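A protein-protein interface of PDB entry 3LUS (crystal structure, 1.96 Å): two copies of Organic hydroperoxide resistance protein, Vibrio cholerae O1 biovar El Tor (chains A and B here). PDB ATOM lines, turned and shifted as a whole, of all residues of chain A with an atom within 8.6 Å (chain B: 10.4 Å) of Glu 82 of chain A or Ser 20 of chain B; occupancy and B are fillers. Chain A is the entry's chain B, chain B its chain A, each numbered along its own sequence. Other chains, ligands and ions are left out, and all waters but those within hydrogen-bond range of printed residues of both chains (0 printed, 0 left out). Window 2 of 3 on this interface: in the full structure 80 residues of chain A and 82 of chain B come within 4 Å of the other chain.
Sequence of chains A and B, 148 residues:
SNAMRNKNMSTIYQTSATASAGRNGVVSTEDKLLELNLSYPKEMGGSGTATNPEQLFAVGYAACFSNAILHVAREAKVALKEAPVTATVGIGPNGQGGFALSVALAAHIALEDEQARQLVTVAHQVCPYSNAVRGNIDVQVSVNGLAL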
ATOM      1  N   VAL A  59      14.055   1.479 -21.009  1.00  0.00           N
ATOM      2  CA  VAL A  59      14.800   0.230 -20.779  1.00  0.00           C
ATOM      3  C   VAL A  59      14.100  -0.900 -21.509  1.00  0.00           C
ATOM      4  O   VAL A  59      14.745  -1.731 -22.156  1.00  0.00           O
ATOM      5  CB  VAL A  59      14.861  -0.026 -19.252  1.00  0.00           C
ATOM      6  CG1 VAL A  59      15.162  -1.449 -18.882  1.00  0.00           C
ATOM      7  CG2 VAL A  59      15.901   0.845 -18.648  1.00  0.00           C
ATOM      8  N   ALA A  62      14.492  -0.367 -25.473  1.00  0.00           N
ATOM      9  CA  ALA A  62      15.887  -0.663 -25.837  1.00  0.00           C
ATOM     10  C   ALA A  62      16.194  -2.183 -25.833  1.00  0.00           C
ATOM     11  O   ALA A  62      16.847  -2.699 -26.779  1.00  0.00           O
ATOM     12  CB  ALA A  62      16.858   0.095 -24.907  1.00  0.00           C
ATOM     13  N   ALA A  63      15.821  -2.888 -24.751  1.00  0.00           N
ATOM     14  CA  ALA A  63      16.079  -4.341 -24.692  1.00  0.00           C
ATOM     15  C   ALA A  63      15.273  -5.103 -25.799  1.00  0.00           C
ATOM     16  O   ALA A  63      15.780  -5.973 -26.485  1.00  0.00           O
ATOM     17  CB  ALA A  63      15.752  -4.905 -23.310  1.00  0.00           C
ATOM     18  N   CYS A  64      14.014  -4.776 -25.948  1.00  0.00           N
ATOM     19  CA  CYS A  64      13.154  -5.429 -26.942  1.00  0.00           C
ATOM     20  C   CYS A  64      13.661  -5.265 -28.377  1.00  0.00           C
ATOM     21  O   CYS A  64      13.700  -6.203 -29.204  1.00  0.00           O
ATOM     22  CB  CYS A  64      11.756  -4.865 -26.815  1.00  0.00           C
ATOM     23  SG  CYS A  64      10.631  -5.965 -27.668  1.00  0.00           S
ATOM     24  N   PHE A  65      14.017  -4.044 -28.690  1.00  0.00           N
ATOM     25  CA  PHE A  65      14.578  -3.734 -30.010  1.00  0.00           C
ATOM     26  C   PHE A  65      15.935  -4.327 -30.266  1.00  0.00           C
ATOM     27  O   PHE A  65      16.155  -4.826 -31.357  1.00  0.00           O
ATOM     28  CB  PHE A  65      14.646  -2.237 -30.228  1.00  0.00           C
ATOM     29  CG  PHE A  65      14.726  -1.839 -31.671  1.00  0.00           C
ATOM     30  CD1 PHE A  65      13.677  -2.033 -32.505  1.00  0.00           C
ATOM     31  CD2 PHE A  65      15.843  -1.194 -32.170  1.00  0.00           C
ATOM     32  CE1 PHE A  65      13.759  -1.660 -33.842  1.00  0.00           C
ATOM     33  CE2 PHE A  65      15.908  -0.773 -33.468  1.00  0.00           C
ATOM     34  CZ  PHE A  65      14.899  -1.025 -34.307  1.00  0.00           C
ATOM     35  N   SER A  66      16.847  -4.288 -29.298  1.00  0.00           N
ATOM     36  CA  SER A  66      18.108  -5.033 -29.406  1.00  0.00           C
ATOM     37  C   SER A  66      17.831  -6.529 -29.692  1.00  0.00           C
ATOM     38  O   SER A  66      18.391  -7.098 -30.633  1.00  0.00           O
ATOM     39  CB  SER A  66      18.956  -4.854 -28.135  1.00  0.00           C
ATOM     40  OG  SER A  66      20.117  -5.616 -28.136  1.00  0.00           O
ATOM     41  N   ASN A  67      16.897  -7.146 -28.970  1.00  0.00           N
ATOM     42  CA  ASN A  67      16.648  -8.512 -29.192  1.00  0.00           C
ATOM     43  C   ASN A  67      16.093  -8.753 -30.591  1.00  0.00           C
ATOM     44  O   ASN A  67      16.346  -9.783 -31.213  1.00  0.00           O
ATOM     45  CB  ASN A  67      15.635  -9.013 -28.202  1.00  0.00           C
ATOM     46  CG  ASN A  67      15.640 -10.475 -28.107  1.00  0.00           C
ATOM     47  OD1 ASN A  67      16.526 -11.019 -27.453  1.00  0.00           O
ATOM     48  ND2 ASN A  67      14.628 -11.149 -28.692  1.00  0.00           N
ATOM     49  N   ILE A  69      16.670  -7.151 -33.284  1.00  0.00           N
ATOM     50  CA  ILE A  69      17.794  -7.128 -34.218  1.00  0.00           C
ATOM     51  C   ILE A  69      18.600  -8.445 -34.195  1.00  0.00           C
ATOM     52  O   ILE A  69      18.914  -9.022 -35.257  1.00  0.00           O
ATOM     53  CB  ILE A  69      18.759  -5.889 -33.960  1.00  0.00           C
ATOM     54  CG1 ILE A  69      18.029  -4.571 -34.314  1.00  0.00           C
ATOM     55  CG2 ILE A  69      20.122  -5.993 -34.805  1.00  0.00           C
ATOM     56  CD1 ILE A  69      18.672  -3.340 -33.759  1.00  0.00           C
ATOM     57  N   LEU A  70      18.961  -8.914 -32.994  1.00  0.00           N
ATOM     58  CA  LEU A  70      19.666 -10.194 -32.881  1.00  0.00           C
ATOM     59  C   LEU A  70      18.841 -11.349 -33.430  1.00  0.00           C
ATOM     60  O   LEU A  70      19.349 -12.283 -34.072  1.00  0.00           O
ATOM     61  CB  LEU A  70      20.028 -10.450 -31.438  1.00  0.00           C
ATOM     62  CG  LEU A  70      21.090  -9.489 -30.896  1.00  0.00           C
ATOM     63  CD1 LEU A  70      21.155  -9.565 -29.319  1.00  0.00           C
ATOM     64  CD2 LEU A  70      22.497  -9.814 -31.558  1.00  0.00           C
ATOM     65  N   ALA A  73      19.076 -11.108 -37.237  1.00  0.00           N
ATOM     66  CA  ALA A  73      20.414 -11.459 -37.657  1.00  0.00           C
ATOM     67  C   ALA A  73      20.640 -12.954 -37.578  1.00  0.00           C
ATOM     68  O   ALA A  73      21.278 -13.496 -38.406  1.00  0.00           O
ATOM     69  CB  ALA A  73      21.428 -10.756 -36.861  1.00  0.00           C
ATOM     70  N   VAL A  78      23.456 -13.783 -40.194  1.00  0.00           N
ATOM     71  CA  VAL A  78      24.433 -12.683 -40.167  1.00  0.00           C
ATOM     72  C   VAL A  78      25.081 -12.726 -38.776  1.00  0.00           C
ATOM     73  O   VAL A  78      24.376 -12.662 -37.776  1.00  0.00           O
ATOM     74  CB  VAL A  78      23.729 -11.336 -40.446  1.00  0.00           C
ATOM     75  CG1 VAL A  78      24.658 -10.110 -40.156  1.00  0.00           C
ATOM     76  CG2 VAL A  78      23.226 -11.296 -41.923  1.00  0.00           C
ATOM     77  N   ALA A  79      26.407 -12.837 -38.675  1.00  0.00           N
ATOM     78  CA  ALA A  79      27.018 -12.979 -37.337  1.00  0.00           C
ATOM     79  C   ALA A  79      27.022 -11.604 -36.684  1.00  0.00           C
ATOM     80  O   ALA A  79      27.579 -10.662 -37.238  1.00  0.00           O
ATOM     81  CB  ALA A  79      28.439 -13.553 -37.414  1.00  0.00           C
ATOM     82  N   LEU A  80      26.285 -11.446 -35.591  1.00  0.00           N
ATOM     83  CA  LEU A  80      26.426 -10.275 -34.730  1.00  0.00           C
ATOM     84  C   LEU A  80      26.750 -10.778 -33.353  1.00  0.00           C
ATOM     85  O   LEU A  80      26.103 -11.673 -32.871  1.00  0.00           O
ATOM     86  CB  LEU A  80      25.119  -9.475 -34.675  1.00  0.00           C
ATOM     87  CG  LEU A  80      24.897  -8.184 -35.411  1.00  0.00           C
ATOM     88  CD1 LEU A  80      25.554  -8.102 -36.826  1.00  0.00           C
ATOM     89  CD2 LEU A  80      23.349  -7.925 -35.457  1.00  0.00           C
ATOM     90  N   LYS A  81      27.714 -10.179 -32.685  1.00  0.00           N
ATOM     91  CA  LYS A  81      28.017 -10.595 -31.302  1.00  0.00           C
ATOM     92  C   LYS A  81      26.987  -9.990 -30.357  1.00  0.00           C
ATOM     93  O   LYS A  81      26.749 -10.499 -29.254  1.00  0.00           O
ATOM     94  CB  LYS A  81      29.426 -10.141 -30.873  1.00  0.00           C
ATOM     95  CG  LYS A  81      30.578 -11.010 -31.369  1.00  0.00           C
ATOM     96  CD  LYS A  81      31.719 -11.120 -30.326  1.00  0.00           C
ATOM     97  CE  LYS A  81      32.636 -12.260 -30.694  1.00  0.00           C
ATOM     98  NZ  LYS A  81      32.864 -12.228 -32.171  1.00  0.00           N
ATOM     99  N   GLU A  82      26.401  -8.877 -30.788  1.00  0.00           N
ATOM    100  CA  GLU A  82      25.633  -7.995 -29.947  1.00  0.00           C
ATOM    101  C   GLU A  82      24.984  -6.896 -30.811  1.00  0.00           C
ATOM    102  O   GLU A  82      25.369  -6.674 -31.968  1.00  0.00           O
ATOM    103  CB  GLU A  82      26.484  -7.346 -28.889  1.00  0.00           C
ATOM    104  CG  GLU A  82      27.573  -6.469 -29.456  1.00  0.00           C
ATOM    105  CD  GLU A  82      28.384  -5.763 -28.368  1.00  0.00           C
ATOM    106  OE1 GLU A  82      29.249  -4.934 -28.724  1.00  0.00           O
ATOM    107  OE2 GLU A  82      28.131  -5.999 -27.158  1.00  0.00           O
ATOM    108  N   ALA A  83      24.015  -6.221 -30.227  1.00  0.00           N
ATOM    109  CA  ALA A  83      23.222  -5.199 -30.939  1.00  0.00           C
ATOM    110  C   ALA A  83      22.909  -4.028 -29.984  1.00  0.00           C
ATOM    111  O   ALA A  83      21.812  -3.951 -29.437  1.00  0.00           O
ATOM    112  CB  ALA A  83      21.885  -5.843 -31.482  1.00  0.00           C
ATOM    113  N   PRO A  84      23.887  -3.117 -29.757  1.00  0.00           N
ATOM    114  CA  PRO A  84      23.659  -1.981 -28.860  1.00  0.00           C
ATOM    115  C   PRO A  84      22.594  -1.108 -29.415  1.00  0.00           C
ATOM    116  O   PRO A  84      22.658  -0.742 -30.609  1.00  0.00           O
ATOM    117  CB  PRO A  84      25.008  -1.238 -28.865  1.00  0.00           C
ATOM    118  CG  PRO A  84      25.981  -2.337 -29.168  1.00  0.00           C
ATOM    119  CD  PRO A  84      25.291  -3.232 -30.135  1.00  0.00           C
ATOM    120  N   VAL A  85      21.607  -0.817 -28.576  1.00  0.00           N
ATOM    121  CA  VAL A  85      20.521   0.099 -28.910  1.00  0.00           C
ATOM    122  C   VAL A  85      20.365   1.067 -27.772  1.00  0.00           C
ATOM    123  O   VAL A  85      20.286   0.642 -26.587  1.00  0.00           O
ATOM    124  CB  VAL A  85      19.168  -0.612 -29.122  1.00  0.00           C
ATOM    125  CG1 VAL A  85      18.049   0.424 -29.350  1.00  0.00           C
ATOM    126  CG2 VAL A  85      19.240  -1.550 -30.347  1.00  0.00           C
ATOM    127  N   THR A  86      20.345   2.360 -28.113  1.00  0.00           N
ATOM    128  CA  THR A  86      19.992   3.406 -27.162  1.00  0.00           C
ATOM    129  C   THR A  86      18.573   3.873 -27.467  1.00  0.00           C
ATOM    130  O   THR A  86      18.308   4.294 -28.601  1.00  0.00           O
ATOM    131  CB  THR A  86      20.928   4.579 -27.274  1.00  0.00           C
ATOM    132  OG1 THR A  86      22.245   4.124 -26.944  1.00  0.00           O
ATOM    133  CG2 THR A  86      20.485   5.705 -26.287  1.00  0.00           C
ATOM    134  N   ALA A 107      20.487   2.356 -33.117  1.00  0.00           N
ATOM    135  CA  ALA A 107      21.208   1.073 -33.124  1.00  0.00           C
ATOM    136  C   ALA A 107      22.657   1.276 -33.558  1.00  0.00           C
ATOM    137  O   ALA A 107      22.931   2.075 -34.450  1.00  0.00           O
ATOM    138  CB  ALA A 107      20.526   0.104 -34.045  1.00  0.00           C
ATOM    139  N   HIS A 108      23.580   0.557 -32.948  1.00  0.00           N
ATOM    140  CA  HIS A 108      24.985   0.605 -33.374  1.00  0.00           C
ATOM    141  C   HIS A 108      25.472  -0.839 -33.598  1.00  0.00           C
ATOM    142  O   HIS A 108      25.793  -1.545 -32.613  1.00  0.00           O
ATOM    143  CB  HIS A 108      25.858   1.350 -32.339  1.00  0.00           C
ATOM    144  CG  HIS A 108      25.146   2.457 -31.593  1.00  0.00           C
ATOM    145  ND1 HIS A 108      25.010   3.734 -32.098  1.00  0.00           N
ATOM    146  CD2 HIS A 108      24.543   2.471 -30.373  1.00  0.00           C
ATOM    147  CE1 HIS A 108      24.323   4.475 -31.242  1.00  0.00           C
ATOM    148  NE2 HIS A 108      24.042   3.739 -30.176  1.00  0.00           N
ATOM    149  N   ILE A 109      25.475  -1.296 -34.864  1.00  0.00           N
ATOM    150  CA  ILE A 109      25.817  -2.667 -35.209  1.00  0.00           C
ATOM    151  C   ILE A 109      26.894  -2.821 -36.290  1.00  0.00           C
ATOM    152  O   ILE A 109      27.120  -1.890 -37.037  1.00  0.00           O
ATOM    153  CB  ILE A 109      24.598  -3.489 -35.637  1.00  0.00           C
ATOM    154  CG1 ILE A 109      24.180  -3.154 -37.054  1.00  0.00           C
ATOM    155  CG2 ILE A 109      23.385  -3.285 -34.595  1.00  0.00           C
ATOM    156  CD1 ILE A 109      22.779  -3.743 -37.436  1.00  0.00           C
ATOM    157  N   ALA A 110      27.444  -4.041 -36.415  1.00  0.00           N
ATOM    158  CA  ALA A 110      28.564  -4.381 -37.413  1.00  0.00           C
ATOM    159  C   ALA A 110      28.051  -4.927 -38.741  1.00  0.00           C
ATOM    160  O   ALA A 110      28.308  -6.097 -39.115  1.00  0.00           O
ATOM    161  CB  ALA A 110      29.479  -5.412 -36.828  1.00  0.00           C
ATOM    162  N   LEU A 111      27.321  -4.099 -39.439  1.00  0.00           N
ATOM    163  CA  LEU A 111      26.650  -4.439 -40.707  1.00  0.00           C
ATOM    164  C   LEU A 111      26.255  -3.059 -41.285  1.00  0.00           C
ATOM    165  O   LEU A 111      25.856  -2.178 -40.490  1.00  0.00           O
ATOM    166  CB  LEU A 111      25.368  -5.259 -40.443  1.00  0.00           C
ATOM    167  CG  LEU A 111      24.611  -5.852 -41.661  1.00  0.00           C
ATOM    168  CD1 LEU A 111      25.324  -7.122 -42.276  1.00  0.00           C
ATOM    169  CD2 LEU A 111      23.152  -6.177 -41.280  1.00  0.00           C
ATOM    170  N   ALA B  17      18.137   4.979 -22.374  1.00  0.00           N
ATOM    171  CA  ALA B  17      18.628   3.703 -21.859  1.00  0.00           C
ATOM    172  C   ALA B  17      19.316   2.960 -22.973  1.00  0.00           C
ATOM    173  O   ALA B  17      18.924   3.085 -24.176  1.00  0.00           O
ATOM    174  CB  ALA B  17      17.464   2.803 -21.246  1.00  0.00           C
ATOM    175  N   THR B  18      20.274   2.122 -22.593  1.00  0.00           N
ATOM    176  CA  THR B  18      21.001   1.327 -23.597  1.00  0.00           C
ATOM    177  C   THR B  18      20.989  -0.137 -23.231  1.00  0.00           C
ATOM    178  O   THR B  18      21.149  -0.455 -22.074  1.00  0.00           O
ATOM    179  CB  THR B  18      22.491   1.812 -23.755  1.00  0.00           C
ATOM    180  OG1 THR B  18      22.511   3.174 -24.220  1.00  0.00           O
ATOM    181  CG2 THR B  18      23.202   0.980 -24.797  1.00  0.00           C
ATOM    182  N   ALA B  19      20.752  -1.002 -24.210  1.00  0.00           N
ATOM    183  CA  ALA B  19      20.868  -2.461 -24.077  1.00  0.00           C
ATOM    184  C   ALA B  19      21.679  -2.992 -25.233  1.00  0.00           C
ATOM    185  O   ALA B  19      21.529  -2.512 -26.359  1.00  0.00           O
ATOM    186  CB  ALA B  19      19.433  -3.147 -24.097  1.00  0.00           C
ATOM    187  N   SER B  20      22.459  -4.057 -25.030  1.00  0.00           N
ATOM    188  CA  SER B  20      23.151  -4.627 -26.186  1.00  0.00           C
ATOM    189  C   SER B  20      22.983  -6.143 -26.433  1.00  0.00           C
ATOM    190  O   SER B  20      23.441  -6.689 -27.504  1.00  0.00           O
ATOM    191  CB  SER B  20      24.625  -4.243 -26.072  1.00  0.00           C
ATOM    192  OG  SER B  20      25.179  -4.892 -24.972  1.00  0.00           O
ATOM    193  N   ALA B  21      22.381  -6.865 -25.490  1.00  0.00           N
ATOM    194  CA  ALA B  21      22.315  -8.371 -25.624  1.00  0.00           C
ATOM    195  C   ALA B  21      20.869  -8.727 -25.609  1.00  0.00           C
ATOM    196  O   ALA B  21      20.472  -9.786 -25.099  1.00  0.00           O
ATOM    197  CB  ALA B  21      23.088  -9.118 -24.486  1.00  0.00           C
ATOM    198  N   GLY B  22      20.069  -7.830 -26.173  1.00  0.00           N
ATOM    199  CA  GLY B  22      18.596  -7.987 -26.177  1.00  0.00           C
ATOM    200  C   GLY B  22      17.971  -8.372 -24.818  1.00  0.00           C
ATOM    201  O   GLY B  22      18.254  -7.736 -23.795  1.00  0.00           O
ATOM    202  N   ARG B  23      17.181  -9.447 -24.824  1.00  0.00           N
ATOM    203  CA  ARG B  23      16.409  -9.939 -23.652  1.00  0.00           C
ATOM    204  C   ARG B  23      17.234 -10.703 -22.624  1.00  0.00           C
ATOM    205  O   ARG B  23      16.688 -11.186 -21.617  1.00  0.00           O
ATOM    206  CB  ARG B  23      15.283 -10.875 -24.151  1.00  0.00           C
ATOM    207  CG  ARG B  23      14.097 -10.155 -24.894  1.00  0.00           C
ATOM    208  CD  ARG B  23      13.103 -11.130 -25.674  1.00  0.00           C
ATOM    209  NE  ARG B  23      11.999 -10.326 -26.198  1.00  0.00           N
ATOM    210  CZ  ARG B  23      10.869 -10.078 -25.539  1.00  0.00           C
ATOM    211  NH1 ARG B  23      10.619 -10.663 -24.359  1.00  0.00           N
ATOM    212  NH2 ARG B  23       9.943  -9.311 -26.096  1.00  0.00           N
ATOM    213  N   ASN B  24      18.531 -10.871 -22.878  1.00  0.00           N
ATOM    214  CA  ASN B  24      19.355 -11.776 -22.064  1.00  0.00           C
ATOM    215  C   ASN B  24      20.726 -11.159 -21.696  1.00  0.00           C
ATOM    216  O   ASN B  24      21.777 -11.755 -21.919  1.00  0.00           O
ATOM    217  CB  ASN B  24      19.494 -13.149 -22.793  1.00  0.00           C
ATOM    218  CG  ASN B  24      19.442 -14.358 -21.834  1.00  0.00           C
ATOM    219  OD1 ASN B  24      19.126 -14.213 -20.649  1.00  0.00           O
ATOM    220  ND2 ASN B  24      19.765 -15.572 -22.361  1.00  0.00           N
ATOM    221  N   GLY B  25      20.692  -9.954 -21.115  1.00  0.00           N
ATOM    222  CA  GLY B  25      21.894  -9.247 -20.615  1.00  0.00           C
ATOM    223  C   GLY B  25      21.499  -8.024 -19.798  1.00  0.00           C
ATOM    224  O   GLY B  25      20.403  -7.958 -19.249  1.00  0.00           O
ATOM    225  N   VAL B  26      22.351  -7.014 -19.761  1.00  0.00           N
ATOM    226  CA  VAL B  26      22.112  -5.862 -18.908  1.00  0.00           C
ATOM    227  C   VAL B  26      21.439  -4.773 -19.680  1.00  0.00           C
ATOM    228  O   VAL B  26      21.544  -4.749 -20.893  1.00  0.00           O
ATOM    229  CB  VAL B  26      23.406  -5.350 -18.300  1.00  0.00           C
ATOM    230  CG1 VAL B  26      23.092  -4.274 -17.220  1.00  0.00           C
ATOM    231  CG2 VAL B  26      24.143  -6.500 -17.707  1.00  0.00           C
ATOM    232  N   VAL B  27      20.656  -3.948 -18.973  1.00  0.00           N
ATOM    233  CA  VAL B  27      20.015  -2.769 -19.533  1.00  0.00           C
ATOM    234  C   VAL B  27      20.036  -1.686 -18.448  1.00  0.00           C
ATOM    235  O   VAL B  27      19.865  -1.961 -17.253  1.00  0.00           O
ATOM    236  CB  VAL B  27      18.603  -3.024 -20.156  1.00  0.00           C
ATOM    237  CG1 VAL B  27      17.535  -3.375 -19.136  1.00  0.00           C
ATOM    238  CG2 VAL B  27      18.140  -1.752 -20.905  1.00  0.00           C
ATOM    239  N   SER B  28      20.345  -0.472 -18.849  1.00  0.00           N
ATOM    240  CA  SER B  28      20.505   0.593 -17.884  1.00  0.00           C
ATOM    241  C   SER B  28      20.145   1.951 -18.463  1.00  0.00           C
ATOM    242  O   SER B  28      20.369   2.215 -19.663  1.00  0.00           O
ATOM    243  CB  SER B  28      21.937   0.547 -17.348  1.00  0.00           C
ATOM    244  OG  SER B  28      22.874   0.860 -18.354  1.00  0.00           O
ATOM    245  N   LEU B  36      19.395  -2.902 -14.690  1.00  0.00           N
ATOM    246  CA  LEU B  36      18.705  -4.162 -14.545  1.00  0.00           C
ATOM    247  C   LEU B  36      19.314  -5.300 -15.352  1.00  0.00           C
ATOM    248  O   LEU B  36      19.875  -5.105 -16.466  1.00  0.00           O
ATOM    249  CB  LEU B  36      17.279  -3.985 -15.023  1.00  0.00           C
ATOM    250  CG  LEU B  36      16.351  -3.132 -14.168  1.00  0.00           C
ATOM    251  CD1 LEU B  36      15.077  -2.891 -14.935  1.00  0.00           C
ATOM    252  CD2 LEU B  36      16.058  -3.776 -12.768  1.00  0.00           C
ATOM    253  N   LEU B  38      18.335  -8.689 -17.396  1.00  0.00           N
ATOM    254  CA  LEU B  38      17.209  -9.302 -18.077  1.00  0.00           C
ATOM    255  C   LEU B  38      17.531 -10.767 -18.431  1.00  0.00           C
ATOM    256  O   LEU B  38      18.675 -11.126 -18.736  1.00  0.00           O
ATOM    257  CB  LEU B  38      16.881  -8.595 -19.397  1.00  0.00           C
ATOM    258  CG  LEU B  38      16.717  -7.078 -19.422  1.00  0.00           C
ATOM    259  CD1 LEU B  38      16.390  -6.621 -20.820  1.00  0.00           C
ATOM    260  CD2 LEU B  38      15.657  -6.646 -18.488  1.00  0.00           C
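The backbone carbonyl oxygen (O) of Ala 19 of chain B lies close to the backbone carbonyl oxygen (O) of Ala 83 of chain A, 3.4 Å away.
The backbone carbonyl oxygen (O) of Ala 19 of chain B sits at hydrogen-bond distance from the backbone NH (N) of Val 85 of chain A, at 2.8 Å.
The backbone NH (N) of Ala 83 of chain A is in hydrogen-bond range of the backbone carbonyl oxygen (O) of Ser 20 of chain B (2.8 Å).
The side-chain sulfur (SG) of Cys 64 of chain A lies within hydrogen-bond range of the guanidinium group (NH2) of Arg 23 of chain B (3.8 Å).
The side-chain hydroxyl (OG1) of Thr 18 of chain B is in hydrogen-bond range of the side-chain hydroxyl (OG1) of Thr 86 of chain A (2.9 Å).
N of Gly 22 of chain B lies within hydrogen-bond range of OG of Ser 66 of chain A (3.0 Å).
The backbone NH (N) of Arg 23 of chain B is in hydrogen-bond range of the side-chain amide oxygen (OD1) of Asn 67 of chain A, at 3.1 Å.
Among the printed residues, pairs that only touch across the chains: Val 59 of chain A with Ala 17 of chain B (3.6 Å), Val 59 of chain A with Val 27 of chain B (3.1 Å), Ala 62 of chain A with Ala 17 of chain B (3.7 Å), Ala 62 of chain A with Ala 19 of chain B (3.8 Å), Ala 63 of chain A with Ala 19 of chain B (3.6 Å), Ala 63 of chain A with Gly 22 of chain B (3.5 Å), Ala 63 of chain A with Leu 38 of chain B (3.1 Å), Ser 66 of chain A with Ala 19 of chain B (3.8 Å), Ser 66 of chain A with Ser 20 of chain B (3.4 Å), Ser 66 of chain A with Ala 21 of chain B (3.7 Å), Asn 67 of chain A with Gly 22 of chain B (3.4 Å), Leu 70 of chain A with Ala 21 of chain B (3.8 Å), Leu 70 of chain A with Gly 22 of chain B (3.8 Å), Glu 82 of chain A with Ser 20 of chain B (3.4 Å), Pro 84 of chain A with Ala 19 of chain B (3.3 Å), Pro 84 of chain A with Ser 20 of chain B (3.7 Å), Val 85 of chain A with Ala 17 of chain B (3.7 Å), Val 85 of chain A with Thr 18 of chain B (3.1 Å) and Thr 86 of chain A with Ala 17 of chain B (3.2 Å).
O of Val 27 of chain B sits at hydrogen-bond distance from N of Leu 36 of chain B.
The backbone carbonyl oxygen of Gly 25 of chain B lies within hydrogen-bond range of the backbone NH of Leu 38 of chain B, 2.9 Å away.
The backbone carbonyl oxygen (O) of Ser 28 of chain B lies within hydrogen-bond range of the backbone NH (N) of Thr 18 of chain B, 2.9 Å away.
The backbone NH (N) of His 108 of chain A sits at hydrogen-bond distance from the backbone carbonyl oxygen (O) of Pro 84 of chain A (2.8 Å).
The side-chain hydroxyl (OG) of Ser 66 of chain A sits at hydrogen-bond distance from the backbone carbonyl oxygen (O) of Ala 83 of chain A (2.7 Å).
No position is printed for both chains.
Of the 14 printed residues of chain B, 9 touch a printed residue of chain A.
Printed residues of chain B that touch a printed residue of chain A: Ala 17, Thr 18, Ala 19, Ser 20, Ala 21, Gly 22, Arg 23, Val 27 and Leu 38.
Along chain B the printed residues that touch a printed residue of chain A span positions 17 to 38.
Of the 24 printed residues of chain A, 12 touch a printed residue of chain B.
Printed residues of chain A that touch a printed residue of chain B: Val 59, Ala 62, Ala 63, Cys 64, Ser 66, Asn 67, Leu 70, Glu 82, Ala 83, Pro 84, Val 85 and Thr 86.
Among the printed residues, no Asp or Glu carboxylate lies within 4 Å of a Lys or Arg side-chain nitrogen of the other chain.
Val 78 of chain A touches none of the printed residues of chain B.
No residue of chain B comes within 4 Å of Leu 80 of chain A.
Glu 82 of chain A touches just one residue of chain B: Ser 20.
Ala 83 of chain A touches two residues of chain B.
Pro 84 of chain A touches just these residues of chain B: Ala 19 (3.3 Å) and Ser 20 (3.7 Å).
His 108 of chain A touches none of the printed residues of chain B.
Of the printed residues of chain A, Thr 18 of chain B touches Val 85 (3.1 Å) and Thr 86 (2.9 Å).
Of the printed residues of chain A, Ala 19 of chain B touches Ala 62, Ala 63, Ser 66, Ala 83, Pro 84 and Val 85.
Of chain A, only Ser 66, Glu 82, Ala 83 and Pro 84 come within 4 Å of Ser 20 of chain B.
Of the printed residues of chain A, Gly 22 of chain B touches Ala 63 (3.5 Å), Ser 66 (3.0 Å), Asn 67 (3.4 Å) and Leu 70 (3.8 Å).
Of the printed residues of chain A, Arg 23 of chain B touches Cys 64 (3.8 Å) and Asn 67 (3.1 Å).
The nearest residue of chain B that does not touch Glu 82 of chain A is Ala 21 of chain B (5.3 Å).
The nearest residue of chain A that does not touch Ser 20 of chain B is Leu 70 of chain A (4.1 Å).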
